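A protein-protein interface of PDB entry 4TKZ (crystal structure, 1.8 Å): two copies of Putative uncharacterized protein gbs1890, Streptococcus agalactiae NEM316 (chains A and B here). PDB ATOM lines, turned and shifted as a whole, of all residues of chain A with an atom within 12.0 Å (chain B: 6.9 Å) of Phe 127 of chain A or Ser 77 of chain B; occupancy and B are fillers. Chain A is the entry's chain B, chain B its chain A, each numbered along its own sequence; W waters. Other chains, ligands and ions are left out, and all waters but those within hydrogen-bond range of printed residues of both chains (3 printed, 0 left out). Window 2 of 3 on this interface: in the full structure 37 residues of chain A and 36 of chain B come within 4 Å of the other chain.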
ATOM      1  N   HIS A 121     -41.358 -17.769 -13.245  1.00  0.00           N
ATOM      2  CA  HIS A 121     -41.417 -16.437 -12.647  1.00  0.00           C
ATOM      3  C   HIS A 121     -40.710 -16.432 -11.296  1.00  0.00           C
ATOM      4  O   HIS A 121     -39.959 -15.506 -10.958  1.00  0.00           O
ATOM      5  CB  HIS A 121     -42.881 -16.020 -12.456  1.00  0.00           C
ATOM      6  CG  HIS A 121     -43.523 -15.486 -13.695  1.00  0.00           C
ATOM      7  ND1 HIS A 121     -43.227 -14.240 -14.203  1.00  0.00           N
ATOM      8  CD2 HIS A 121     -44.448 -16.021 -14.526  1.00  0.00           C
ATOM      9  CE1 HIS A 121     -43.939 -14.033 -15.297  1.00  0.00           C
ATOM     10  NE2 HIS A 121     -44.680 -15.103 -15.520  1.00  0.00           N
ATOM     11  N   GLU A 122     -40.961 -17.475 -10.522  1.00  0.00           N
ATOM     12  CA  GLU A 122     -40.395 -17.576  -9.188  1.00  0.00           C
ATOM     13  C   GLU A 122     -38.877 -17.714  -9.213  1.00  0.00           C
ATOM     14  O   GLU A 122     -38.199 -17.469  -8.206  1.00  0.00           O
ATOM     15  CB  GLU A 122     -41.023 -18.755  -8.450  1.00  0.00           C
ATOM     16  CG  GLU A 122     -42.445 -18.493  -7.974  1.00  0.00           C
ATOM     17  CD  GLU A 122     -43.057 -19.699  -7.306  1.00  0.00           C
ATOM     18  OE1 GLU A 122     -42.751 -20.833  -7.733  1.00  0.00           O
ATOM     19  OE2 GLU A 122     -43.844 -19.515  -6.356  1.00  0.00           O
ATOM     20  N   GLY A 123     -38.342 -18.116 -10.357  1.00  0.00           N
ATOM     21  CA  GLY A 123     -36.908 -18.324 -10.500  1.00  0.00           C
ATOM     22  C   GLY A 123     -36.119 -17.074 -10.855  1.00  0.00           C
ATOM     23  O   GLY A 123     -34.889 -17.102 -10.901  1.00  0.00           O
ATOM     24  N   ILE A 124     -36.832 -15.986 -11.113  1.00  0.00           N
ATOM     25  CA  ILE A 124     -36.224 -14.684 -11.376  1.00  0.00           C
ATOM     26  C   ILE A 124     -36.124 -13.940 -10.055  1.00  0.00           C
ATOM     27  O   ILE A 124     -37.132 -13.505  -9.488  1.00  0.00           O
ATOM     28  CB  ILE A 124     -37.061 -13.864 -12.374  1.00  0.00           C
ATOM     29  CG1 ILE A 124     -37.159 -14.612 -13.699  1.00  0.00           C
ATOM     30  CG2 ILE A 124     -36.431 -12.493 -12.624  1.00  0.00           C
ATOM     31  CD1 ILE A 124     -38.258 -14.082 -14.634  1.00  0.00           C
ATOM     32  N   VAL A 125     -34.900 -13.813  -9.568  1.00  0.00           N
ATOM     33  CA  VAL A 125     -34.657 -13.280  -8.230  1.00  0.00           C
ATOM     34  C   VAL A 125     -33.453 -12.347  -8.270  1.00  0.00           C
ATOM     35  O   VAL A 125     -32.443 -12.656  -8.910  1.00  0.00           O
ATOM     36  CB  VAL A 125     -34.396 -14.421  -7.218  1.00  0.00           C
ATOM     37  CG1 VAL A 125     -33.920 -13.864  -5.888  1.00  0.00           C
ATOM     38  CG2 VAL A 125     -35.644 -15.259  -7.011  1.00  0.00           C
ATOM     39  N   ASP A 126     -33.571 -11.199  -7.602  1.00  0.00           N
ATOM     40  CA  ASP A 126     -32.445 -10.291  -7.408  1.00  0.00           C
ATOM     41  C   ASP A 126     -31.851 -10.596  -6.031  1.00  0.00           C
ATOM     42  O   ASP A 126     -32.556 -10.535  -5.028  1.00  0.00           O
ATOM     43  CB  ASP A 126     -32.943  -8.842  -7.466  1.00  0.00           C
ATOM     44  CG  ASP A 126     -31.849  -7.808  -7.176  1.00  0.00           C
ATOM     45  OD1 ASP A 126     -30.757  -8.158  -6.670  1.00  0.00           O
ATOM     46  OD2 ASP A 126     -32.101  -6.619  -7.454  1.00  0.00           O
ATOM     47  N   PHE A 127     -30.562 -10.922  -5.982  1.00  0.00           N
ATOM     48  CA  PHE A 127     -29.936 -11.327  -4.726  1.00  0.00           C
ATOM     49  C   PHE A 127     -30.049 -10.259  -3.634  1.00  0.00           C
ATOM     50  O   PHE A 127     -30.077 -10.584  -2.443  1.00  0.00           O
ATOM     51  CB  PHE A 127     -28.476 -11.716  -4.950  1.00  0.00           C
ATOM     52  CG  PHE A 127     -27.726 -11.995  -3.674  1.00  0.00           C
ATOM     53  CD1 PHE A 127     -28.068 -13.080  -2.875  1.00  0.00           C
ATOM     54  CD2 PHE A 127     -26.684 -11.176  -3.279  1.00  0.00           C
ATOM     55  CE1 PHE A 127     -27.379 -13.342  -1.690  1.00  0.00           C
ATOM     56  CE2 PHE A 127     -25.984 -11.430  -2.082  1.00  0.00           C
ATOM     57  CZ  PHE A 127     -26.340 -12.515  -1.299  1.00  0.00           C
ATOM     58  N   SER A 128     -30.122  -8.993  -4.038  1.00  0.00           N
ATOM     59  CA  SER A 128     -30.321  -7.893  -3.092  1.00  0.00           C
ATOM     60  C   SER A 128     -31.559  -8.098  -2.228  1.00  0.00           C
ATOM     61  O   SER A 128     -31.646  -7.579  -1.109  1.00  0.00           O
ATOM     62  CB  SER A 128     -30.457  -6.558  -3.830  1.00  0.00           C
ATOM     63  OG  SER A 128     -29.244  -6.174  -4.443  1.00  0.00           O
ATOM     64  N   THR A 129     -32.497  -8.878  -2.753  1.00  0.00           N
ATOM     65  CA  THR A 129     -33.862  -8.942  -2.235  1.00  0.00           C
ATOM     66  C   THR A 129     -34.035  -9.688  -0.887  1.00  0.00           C
ATOM     67  O   THR A 129     -35.139  -9.758  -0.337  1.00  0.00           O
ATOM     68  CB  THR A 129     -34.859  -9.368  -3.367  1.00  0.00           C
ATOM     69  OG1 THR A 129     -35.882  -8.374  -3.506  1.00  0.00           O
ATOM     70  CG2 THR A 129     -35.464 -10.748  -3.124  1.00  0.00           C
ATOM     71  N   CYS A 130     -32.936 -10.211  -0.349  1.00  0.00           N
ATOM     72  CA  CYS A 130     -32.832 -10.420   1.097  1.00  0.00           C
ATOM     73  C   CYS A 130     -31.537  -9.806   1.624  1.00  0.00           C
ATOM     74  O   CYS A 130     -31.550  -9.010   2.563  1.00  0.00           O
ATOM     75  CB  CYS A 130     -32.913 -11.894   1.498  1.00  0.00           C
ATOM     76  SG  CYS A 130     -32.767 -12.125   3.298  1.00  0.00           S
ATOM     77  N   LEU B  48     -14.807 -15.537 -12.084  1.00  0.00           N
ATOM     78  CA  LEU B  48     -15.590 -14.323 -11.847  1.00  0.00           C
ATOM     79  C   LEU B  48     -14.721 -13.182 -11.340  1.00  0.00           C
ATOM     80  O   LEU B  48     -14.820 -12.065 -11.851  1.00  0.00           O
ATOM     81  CB  LEU B  48     -16.762 -14.586 -10.898  1.00  0.00           C
ATOM     82  CG  LEU B  48     -17.790 -13.464 -10.733  1.00  0.00           C
ATOM     83  CD1 LEU B  48     -18.434 -13.080 -12.086  1.00  0.00           C
ATOM     84  CD2 LEU B  48     -18.870 -13.874  -9.752  1.00  0.00           C
ATOM     85  N   VAL B  60     -24.499  -9.456 -13.150  1.00  0.00           N
ATOM     86  CA  VAL B  60     -24.257 -10.883 -13.307  1.00  0.00           C
ATOM     87  C   VAL B  60     -25.563 -11.641 -13.495  1.00  0.00           C
ATOM     88  O   VAL B  60     -26.438 -11.661 -12.609  1.00  0.00           O
ATOM     89  CB  VAL B  60     -23.510 -11.487 -12.111  1.00  0.00           C
ATOM     90  CG1 VAL B  60     -23.221 -12.955 -12.394  1.00  0.00           C
ATOM     91  CG2 VAL B  60     -22.217 -10.720 -11.834  1.00  0.00           C
ATOM     92  N   LEU B  65     -31.579 -20.067  -9.260  1.00  0.00           N
ATOM     93  CA  LEU B  65     -31.510 -19.708  -7.848  1.00  0.00           C
ATOM     94  C   LEU B  65     -30.993 -20.859  -7.006  1.00  0.00           C
ATOM     95  O   LEU B  65     -31.531 -21.967  -7.050  1.00  0.00           O
ATOM     96  CB  LEU B  65     -32.887 -19.288  -7.338  1.00  0.00           C
ATOM     97  CG  LEU B  65     -32.958 -18.932  -5.855  1.00  0.00           C
ATOM     98  CD1 LEU B  65     -32.167 -17.668  -5.590  1.00  0.00           C
ATOM     99  CD2 LEU B  65     -34.403 -18.775  -5.415  1.00  0.00           C
ATOM    100  N   PHE B  70     -25.043 -18.980  -9.151  1.00  0.00           N
ATOM    101  CA  PHE B  70     -25.704 -17.922  -8.404  1.00  0.00           C
ATOM    102  C   PHE B  70     -25.004 -17.765  -7.049  1.00  0.00           C
ATOM    103  O   PHE B  70     -24.684 -16.649  -6.623  1.00  0.00           O
ATOM    104  CB  PHE B  70     -27.178 -18.255  -8.193  1.00  0.00           C
ATOM    105  CG  PHE B  70     -27.907 -17.257  -7.347  1.00  0.00           C
ATOM    106  CD1 PHE B  70     -28.427 -16.094  -7.904  1.00  0.00           C
ATOM    107  CD2 PHE B  70     -28.069 -17.481  -5.984  1.00  0.00           C
ATOM    108  CE1 PHE B  70     -29.096 -15.169  -7.112  1.00  0.00           C
ATOM    109  CE2 PHE B  70     -28.739 -16.570  -5.188  1.00  0.00           C
ATOM    110  CZ  PHE B  70     -29.249 -15.414  -5.744  1.00  0.00           C
ATOM    111  N   ASN B  71     -24.762 -18.886  -6.383  1.00  0.00           N
ATOM    112  CA  ASN B  71     -24.142 -18.857  -5.051  1.00  0.00           C
ATOM    113  C   ASN B  71     -22.752 -18.214  -5.035  1.00  0.00           C
ATOM    114  O   ASN B  71     -22.453 -17.359  -4.189  1.00  0.00           O
ATOM    115  CB  ASN B  71     -24.068 -20.275  -4.465  1.00  0.00           C
ATOM    116  CG  ASN B  71     -25.438 -20.848  -4.123  1.00  0.00           C
ATOM    117  OD1 ASN B  71     -26.442 -20.135  -4.071  1.00  0.00           O
ATOM    118  ND2 ASN B  71     -25.479 -22.156  -3.887  1.00  0.00           N
ATOM    119  N   VAL B  72     -21.900 -18.634  -5.963  1.00  0.00           N
ATOM    120  CA  VAL B  72     -20.576 -18.033  -6.109  1.00  0.00           C
ATOM    121  C   VAL B  72     -20.668 -16.551  -6.453  1.00  0.00           C
ATOM    122  O   VAL B  72     -19.920 -15.747  -5.914  1.00  0.00           O
ATOM    123  CB  VAL B  72     -19.744 -18.754  -7.188  1.00  0.00           C
ATOM    124  CG1 VAL B  72     -18.563 -17.905  -7.621  1.00  0.00           C
ATOM    125  CG2 VAL B  72     -19.266 -20.101  -6.689  1.00  0.00           C
ATOM    126  N   SER B  73     -21.573 -16.191  -7.364  1.00  0.00           N
ATOM    127  CA  SER B  73     -21.696 -14.798  -7.763  1.00  0.00           C
ATOM    128  C   SER B  73     -22.192 -13.914  -6.617  1.00  0.00           C
ATOM    129  O   SER B  73     -21.677 -12.809  -6.406  1.00  0.00           O
ATOM    130  CB  SER B  73     -22.617 -14.669  -8.981  1.00  0.00           C
ATOM    131  OG  SER B  73     -22.118 -15.459 -10.045  1.00  0.00           O
ATOM    132  N   SER B  74     -23.193 -14.402  -5.888  1.00  0.00           N
ATOM    133  CA  SER B  74     -23.776 -13.666  -4.780  1.00  0.00           C
ATOM    134  C   SER B  74     -22.755 -13.423  -3.672  1.00  0.00           C
ATOM    135  O   SER B  74     -22.695 -12.328  -3.113  1.00  0.00           O
ATOM    136  CB  SER B  74     -24.970 -14.429  -4.206  1.00  0.00           C
ATOM    137  OG  SER B  74     -26.052 -14.422  -5.119  1.00  0.00           O
ATOM    138  N   ALA B  75     -21.964 -14.449  -3.370  1.00  0.00           N
ATOM    139  CA  ALA B  75     -20.960 -14.385  -2.297  1.00  0.00           C
ATOM    140  C   ALA B  75     -19.885 -13.359  -2.604  1.00  0.00           C
ATOM    141  O   ALA B  75     -19.390 -12.666  -1.709  1.00  0.00           O
ATOM    142  CB  ALA B  75     -20.323 -15.748  -2.089  1.00  0.00           C
ATOM    143  N   LEU B  76     -19.511 -13.279  -3.874  1.00  0.00           N
ATOM    144  CA  LEU B  76     -18.463 -12.374  -4.298  1.00  0.00           C
ATOM    145  C   LEU B  76     -18.979 -10.945  -4.395  1.00  0.00           C
ATOM    146  O   LEU B  76     -18.215 -10.001  -4.219  1.00  0.00           O
ATOM    147  CB  LEU B  76     -17.878 -12.826  -5.633  1.00  0.00           C
ATOM    148  CG  LEU B  76     -16.527 -12.217  -5.998  1.00  0.00           C
ATOM    149  CD1 LEU B  76     -15.451 -12.635  -4.986  1.00  0.00           C
ATOM    150  CD2 LEU B  76     -16.131 -12.618  -7.416  1.00  0.00           C
ATOM    151  N   SER B  77     -20.276 -10.784  -4.668  1.00  0.00           N
ATOM    152  CA  SER B  77     -20.856  -9.458  -4.886  1.00  0.00           C
ATOM    153  C   SER B  77     -20.807  -8.550  -3.654  1.00  0.00           C
ATOM    154  O   SER B  77     -21.014  -7.347  -3.770  1.00  0.00           O
ATOM    155  CB  SER B  77     -22.311  -9.574  -5.337  1.00  0.00           C
ATOM    156  OG  SER B  77     -23.126  -9.962  -4.246  1.00  0.00           O
ATOM    157  N   VAL B  78     -20.551  -9.117  -2.482  1.00  0.00           N
ATOM    158  CA  VAL B  78     -20.545  -8.311  -1.258  1.00  0.00           C
ATOM    159  C   VAL B  78     -19.137  -8.073  -0.716  1.00  0.00           C
ATOM    160  O   VAL B  78     -18.974  -7.608   0.418  1.00  0.00           O
ATOM    161  CB  VAL B  78     -21.418  -8.946  -0.155  1.00  0.00           C
ATOM    162  CG1 VAL B  78     -22.827  -9.188  -0.653  1.00  0.00           C
ATOM    163  CG2 VAL B  78     -20.808 -10.256   0.323  1.00  0.00           C
ATOM    164  N   GLU B  79     -18.122  -8.373  -1.519  1.00  0.00           N
ATOM    165  CA  GLU B  79     -16.743  -8.362  -1.018  1.00  0.00           C
ATOM    166  C   GLU B  79     -15.940  -7.150  -1.471  1.00  0.00           C
ATOM    167  O   GLU B  79     -14.857  -6.877  -0.945  1.00  0.00           O
ATOM    168  CB  GLU B  79     -16.013  -9.622  -1.457  1.00  0.00           C
ATOM    169  CG  GLU B  79     -16.576 -10.904  -0.903  1.00  0.00           C
ATOM    170  CD  GLU B  79     -15.499 -11.929  -0.727  1.00  0.00           C
ATOM    171  OE1 GLU B  79     -14.627 -11.696   0.134  1.00  0.00           O
ATOM    172  OE2 GLU B  79     -15.510 -12.944  -1.454  1.00  0.00           O
ATOM    173  N   TYR B  80     -16.465  -6.434  -2.458  1.00  0.00           N
ATOM    174  CA  TYR B  80     -15.804  -5.246  -2.970  1.00  0.00           C
ATOM    175  C   TYR B  80     -16.545  -3.995  -2.501  1.00  0.00           C
ATOM    176  O   TYR B  80     -17.730  -3.816  -2.790  1.00  0.00           O
ATOM    177  CB  TYR B  80     -15.763  -5.277  -4.498  1.00  0.00           C
ATOM    178  CG  TYR B  80     -15.119  -6.502  -5.109  1.00  0.00           C
ATOM    179  CD1 TYR B  80     -15.841  -7.679  -5.283  1.00  0.00           C
ATOM    180  CD2 TYR B  80     -13.800  -6.474  -5.540  1.00  0.00           C
ATOM    181  CE1 TYR B  80     -15.266  -8.791  -5.859  1.00  0.00           C
ATOM    182  CE2 TYR B  80     -13.216  -7.580  -6.126  1.00  0.00           C
ATOM    183  CZ  TYR B  80     -13.954  -8.734  -6.285  1.00  0.00           C
ATOM    184  OH  TYR B  80     -13.369  -9.838  -6.871  1.00  0.00           O
ATOM    185  N   LYS B  83     -17.270  -1.568  -5.777  1.00  0.00           N
ATOM    186  CA  LYS B  83     -17.908  -2.140  -6.955  1.00  0.00           C
ATOM    187  C   LYS B  83     -19.398  -2.275  -6.708  1.00  0.00           C
ATOM    188  O   LYS B  83     -19.829  -2.580  -5.593  1.00  0.00           O
ATOM    189  CB  LYS B  83     -17.334  -3.515  -7.286  1.00  0.00           C
ATOM    190  CG  LYS B  83     -15.871  -3.503  -7.710  1.00  0.00           C
ATOM    191  CD  LYS B  83     -15.475  -4.869  -8.243  1.00  0.00           C
ATOM    192  CE  LYS B  83     -14.003  -4.918  -8.585  1.00  0.00           C
ATOM    193  NZ  LYS B  83     -13.609  -3.840  -9.528  1.00  0.00           N
ATOM    194  N   LYS B  84     -20.183  -2.038  -7.751  1.00  0.00           N
ATOM    195  CA  LYS B  84     -21.612  -2.315  -7.701  1.00  0.00           C
ATOM    196  C   LYS B  84     -21.878  -3.574  -8.518  1.00  0.00           C
ATOM    197  O   LYS B  84     -21.783  -3.558  -9.742  1.00  0.00           O
ATOM    198  CB  LYS B  84     -22.407  -1.124  -8.236  1.00  0.00           C
ATOM    199  CG  LYS B  84     -22.378   0.089  -7.311  1.00  0.00           C
ATOM    200  CD  LYS B  84     -23.141  -0.185  -6.022  1.00  0.00           C
ATOM    201  CE  LYS B  84     -22.757   0.795  -4.916  1.00  0.00           C
ATOM    202  NZ  LYS B  84     -21.459   0.437  -4.269  1.00  0.00           N
ATOM    203  N   ILE B  85     -22.163  -4.675  -7.833  1.00  0.00           N
ATOM    204  CA  ILE B  85     -22.392  -5.949  -8.506  1.00  0.00           C
ATOM    205  C   ILE B  85     -23.801  -6.443  -8.211  1.00  0.00           C
ATOM    206  O   ILE B  85     -24.129  -6.751  -7.068  1.00  0.00           O
ATOM    207  CB  ILE B  85     -21.368  -7.012  -8.078  1.00  0.00           C
ATOM    208  CG1 ILE B  85     -19.944  -6.531  -8.380  1.00  0.00           C
ATOM    209  CG2 ILE B  85     -21.643  -8.334  -8.780  1.00  0.00           C
ATOM    210  CD1 ILE B  85     -18.835  -7.365  -7.726  1.00  0.00           C
ATOM    211  N   LYS B  86     -24.639  -6.493  -9.247  1.00  0.00           N
ATOM    212  CA  LYS B  86     -25.978  -7.045  -9.114  1.00  0.00           C
ATOM    213  C   LYS B  86     -25.982  -8.484  -9.619  1.00  0.00           C
ATOM    214  O   LYS B  86     -25.392  -8.789 -10.658  1.00  0.00           O
ATOM    215  CB  LYS B  86     -26.981  -6.200  -9.915  1.00  0.00           C
ATOM    216  CG  LYS B  86     -27.286  -4.843  -9.284  1.00  0.00           C
ATOM    217  CD  LYS B  86     -28.078  -5.013  -7.990  1.00  0.00           C
ATOM    218  CE  LYS B  86     -28.725  -3.703  -7.550  1.00  0.00           C
ATOM    219  NZ  LYS B  86     -29.118  -3.698  -6.110  1.00  0.00           N
ATOM    220  N   VAL B  87     -26.648  -9.365  -8.881  1.00  0.00           N
ATOM    221  CA  VAL B  87     -26.700 -10.779  -9.232  1.00  0.00           C
ATOM    222  C   VAL B  87     -28.145 -11.222  -9.391  1.00  0.00           C
ATOM    223  O   VAL B  87     -28.918 -11.210  -8.422  1.00  0.00           O
ATOM    224  CB  VAL B  87     -26.031 -11.643  -8.146  1.00  0.00           C
ATOM    225  CG1 VAL B  87     -26.085 -13.122  -8.520  1.00  0.00           C
ATOM    226  CG2 VAL B  87     -24.582 -11.185  -7.921  1.00  0.00           C
ATOM    227  N   LEU B  88     -28.520 -11.609 -10.612  1.00  0.00           N
ATOM    228  CA  LEU B  88     -29.868 -12.118 -10.855  1.00  0.00           C
ATOM    229  C   LEU B  88     -29.847 -13.618 -11.150  1.00  0.00           C
ATOM    230  O   LEU B  88     -28.885 -14.128 -11.727  1.00  0.00           O
ATOM    231  CB  LEU B  88     -30.535 -11.394 -12.040  1.00  0.00           C
ATOM    232  CG  LEU B  88     -30.520  -9.869 -12.088  1.00  0.00           C
ATOM    233  CD1 LEU B  88     -31.419  -9.361 -13.239  1.00  0.00           C
ATOM    234  CD2 LEU B  88     -30.967  -9.290 -10.755  1.00  0.00           C
ATOM    235  N   SER B  89     -30.902 -14.320 -10.733  1.00  0.00           N
ATOM    236  CA  SER B  89     -31.174 -15.673 -11.216  1.00  0.00           C
ATOM    237  C   SER B  89     -32.333 -15.598 -12.215  1.00  0.00           C
ATOM    238  O   SER B  89     -32.939 -14.537 -12.378  1.00  0.00           O
ATOM    239  CB  SER B  89     -31.545 -16.603 -10.072  1.00  0.00           C
ATOM    240  OG  SER B  89     -32.721 -16.164  -9.420  1.00  0.00           O
HETATM  241  O   HOH W   1     -27.871  -8.419  -6.588  1.00  0.00           O
HETATM  242  O   HOH W   2     -33.734 -19.648 -10.789  1.00  0.00           O
HETATM  243  O   HOH W   3     -26.251  -7.002  -5.096  1.00  0.00           O
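Water W2 bridges the backbone NH (N) of Leu 65 of chain B (2.7 Å) and the backbone carbonyl oxygen (O) of Gly 123 of chain A (2.8 Å).
Water W1 lies within hydrogen-bond range of N of Val 87 of chain B (2.8 Å), OD1 of Asp 126 of chain A (2.9 Å) and OG of Ser 128 of chain A (3.4 Å).
Water W3 lies within hydrogen-bond range of the backbone carbonyl oxygen (O) of Ile 85 of chain B (2.9 Å) and the side-chain hydroxyl (OG) of Ser 128 of chain A (3.2 Å).
The backbone NH (N) of Val 60 of chain B lies within hydrogen-bond range of the backbone carbonyl oxygen (O) of Lys 86 of chain B (2.7 Å).
The backbone NH of Leu 88 of chain B lies within hydrogen-bond range of the backbone carbonyl oxygen of Val 60 of chain B, 2.9 Å away.
The backbone carbonyl oxygen (O) of Phe 70 of chain B lies within hydrogen-bond range of the side-chain hydroxyl (OG) of Ser 74 of chain B.
OG of Ser 77 of chain B sits at hydrogen-bond distance from O of Ser 74 of chain B.
N of Ser 128 of chain A lies within hydrogen-bond range of OD1 of Asp 126 of chain A (2.8 Å).
Ser 89 of chain B touches Ile 124 of chain A (O to CA, 3.4 Å).
Val 87 of chain B touches Val 125 of chain A (O to O, 3.8 Å).
Leu 88 of chain B touches Val 125 of chain A.
Val 87 of chain B touches Asp 126 of chain A.
CA of Asp 126 of chain A touches CD2 of Leu 88 of chain B, at 3.8 Å.
CB of Phe 127 of chain A touches CZ of Phe 70 of chain B, at 3.9 Å.
CG of Phe 127 of chain A touches OG of Ser 74 of chain B, 3.3 Å away.
Phe 127 of chain A touches Ser 77 of chain B.
Hydrophobic or aromatic side chains of chain B within 4 Å of the printed part of chain A: Phe 70 and Leu 88.
Of the 10 printed residues of chain A, 6 touch a printed residue of chain B.
Printed residues of chain A that touch a printed residue of chain B: Gly 123, Ile 124, Val 125, Asp 126, Phe 127 and Ser 128.
Hydrophobic or aromatic side chains of chain A that line the printed part of chain B: Val 125 and Phe 127.
Among the printed residues, 12 pairs touch across the chains.
Among the printed residues, no Asp or Glu carboxylate lies within 4 Å of a Lys or Arg side-chain nitrogen of the other chain.
No position is printed for both chains.
Of the 12 pairs that touch across the chains among the printed residues, none has its exchanged pair printed and touching as well.
Printed residues of chain B within 4 Å of Gly 123 of chain A: Ser 89 (2.8 Å).
Of the printed residues of chain B, Ile 124 of chain A touches Ser 89.
Printed residues of chain B within 4 Å of Asp 126 of chain A: Val 87 (3.8 Å) and Leu 88 (3.8 Å).
Phe 127 of chain A touches just these residues of chain B: Phe 70, Ser 74, Ser 77 and Val 87.
Printed residues of chain B within 4 Å of Ser 128 of chain A: Lys 86.
No residue of chain A comes within 4 Å of Ser 73 of chain B.
Of chain A, only Phe 127 comes within 4 Å of Ser 74 of chain B.
No residue of chain A comes within 4 Å of Ala 75 of chain B.
No residue of chain A comes within 4 Å of Leu 76 of chain B.
Ser 77 of chain B touches just one residue of chain A: Phe 127 (3.9 Å).
No residue of chain A comes within 4 Å of Glu 79 of chain B.
Lys 83 of chain B touches none of the printed residues of chain A.
Lys 86 of chain B touches just one residue of chain A: Ser 128 (3.0 Å).
Val 87 of chain B touches just these residues of chain A: Val 125, Asp 126 and Phe 127.
Printed residues of chain A within 4 Å of Ser 89 of chain B: Gly 123 (2.8 Å), Ile 124 (3.4 Å) and Val 125 (2.9 Å).
The nearest residue of chain B that does not touch Phe 127 of chain A is Val 78 of chain B (4.1 Å).
The nearest residue of chain A that does not touch Ser 77 of chain B is Ser 128 of chain A (7.1 Å).
The side-chain hydroxyl (OG) of Ser 128 of chain A is in hydrogen-bond range of the side-chain amino group (NZ) of Lys 86 of chain B (3.0 Å).
The backbone NH of Phe 127 of chain A sits at hydrogen-bond distance from the backbone carbonyl oxygen of Val 87 of chain B, 3.0 Å away.
O of Gly 123 of chain A lies within hydrogen-bond range of OG of Ser 89 of chain B, 2.8 Å away.
The backbone NH of Ser 89 of chain B sits at hydrogen-bond distance from the backbone carbonyl oxygen of Val 125 of chain A (2.9 Å).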
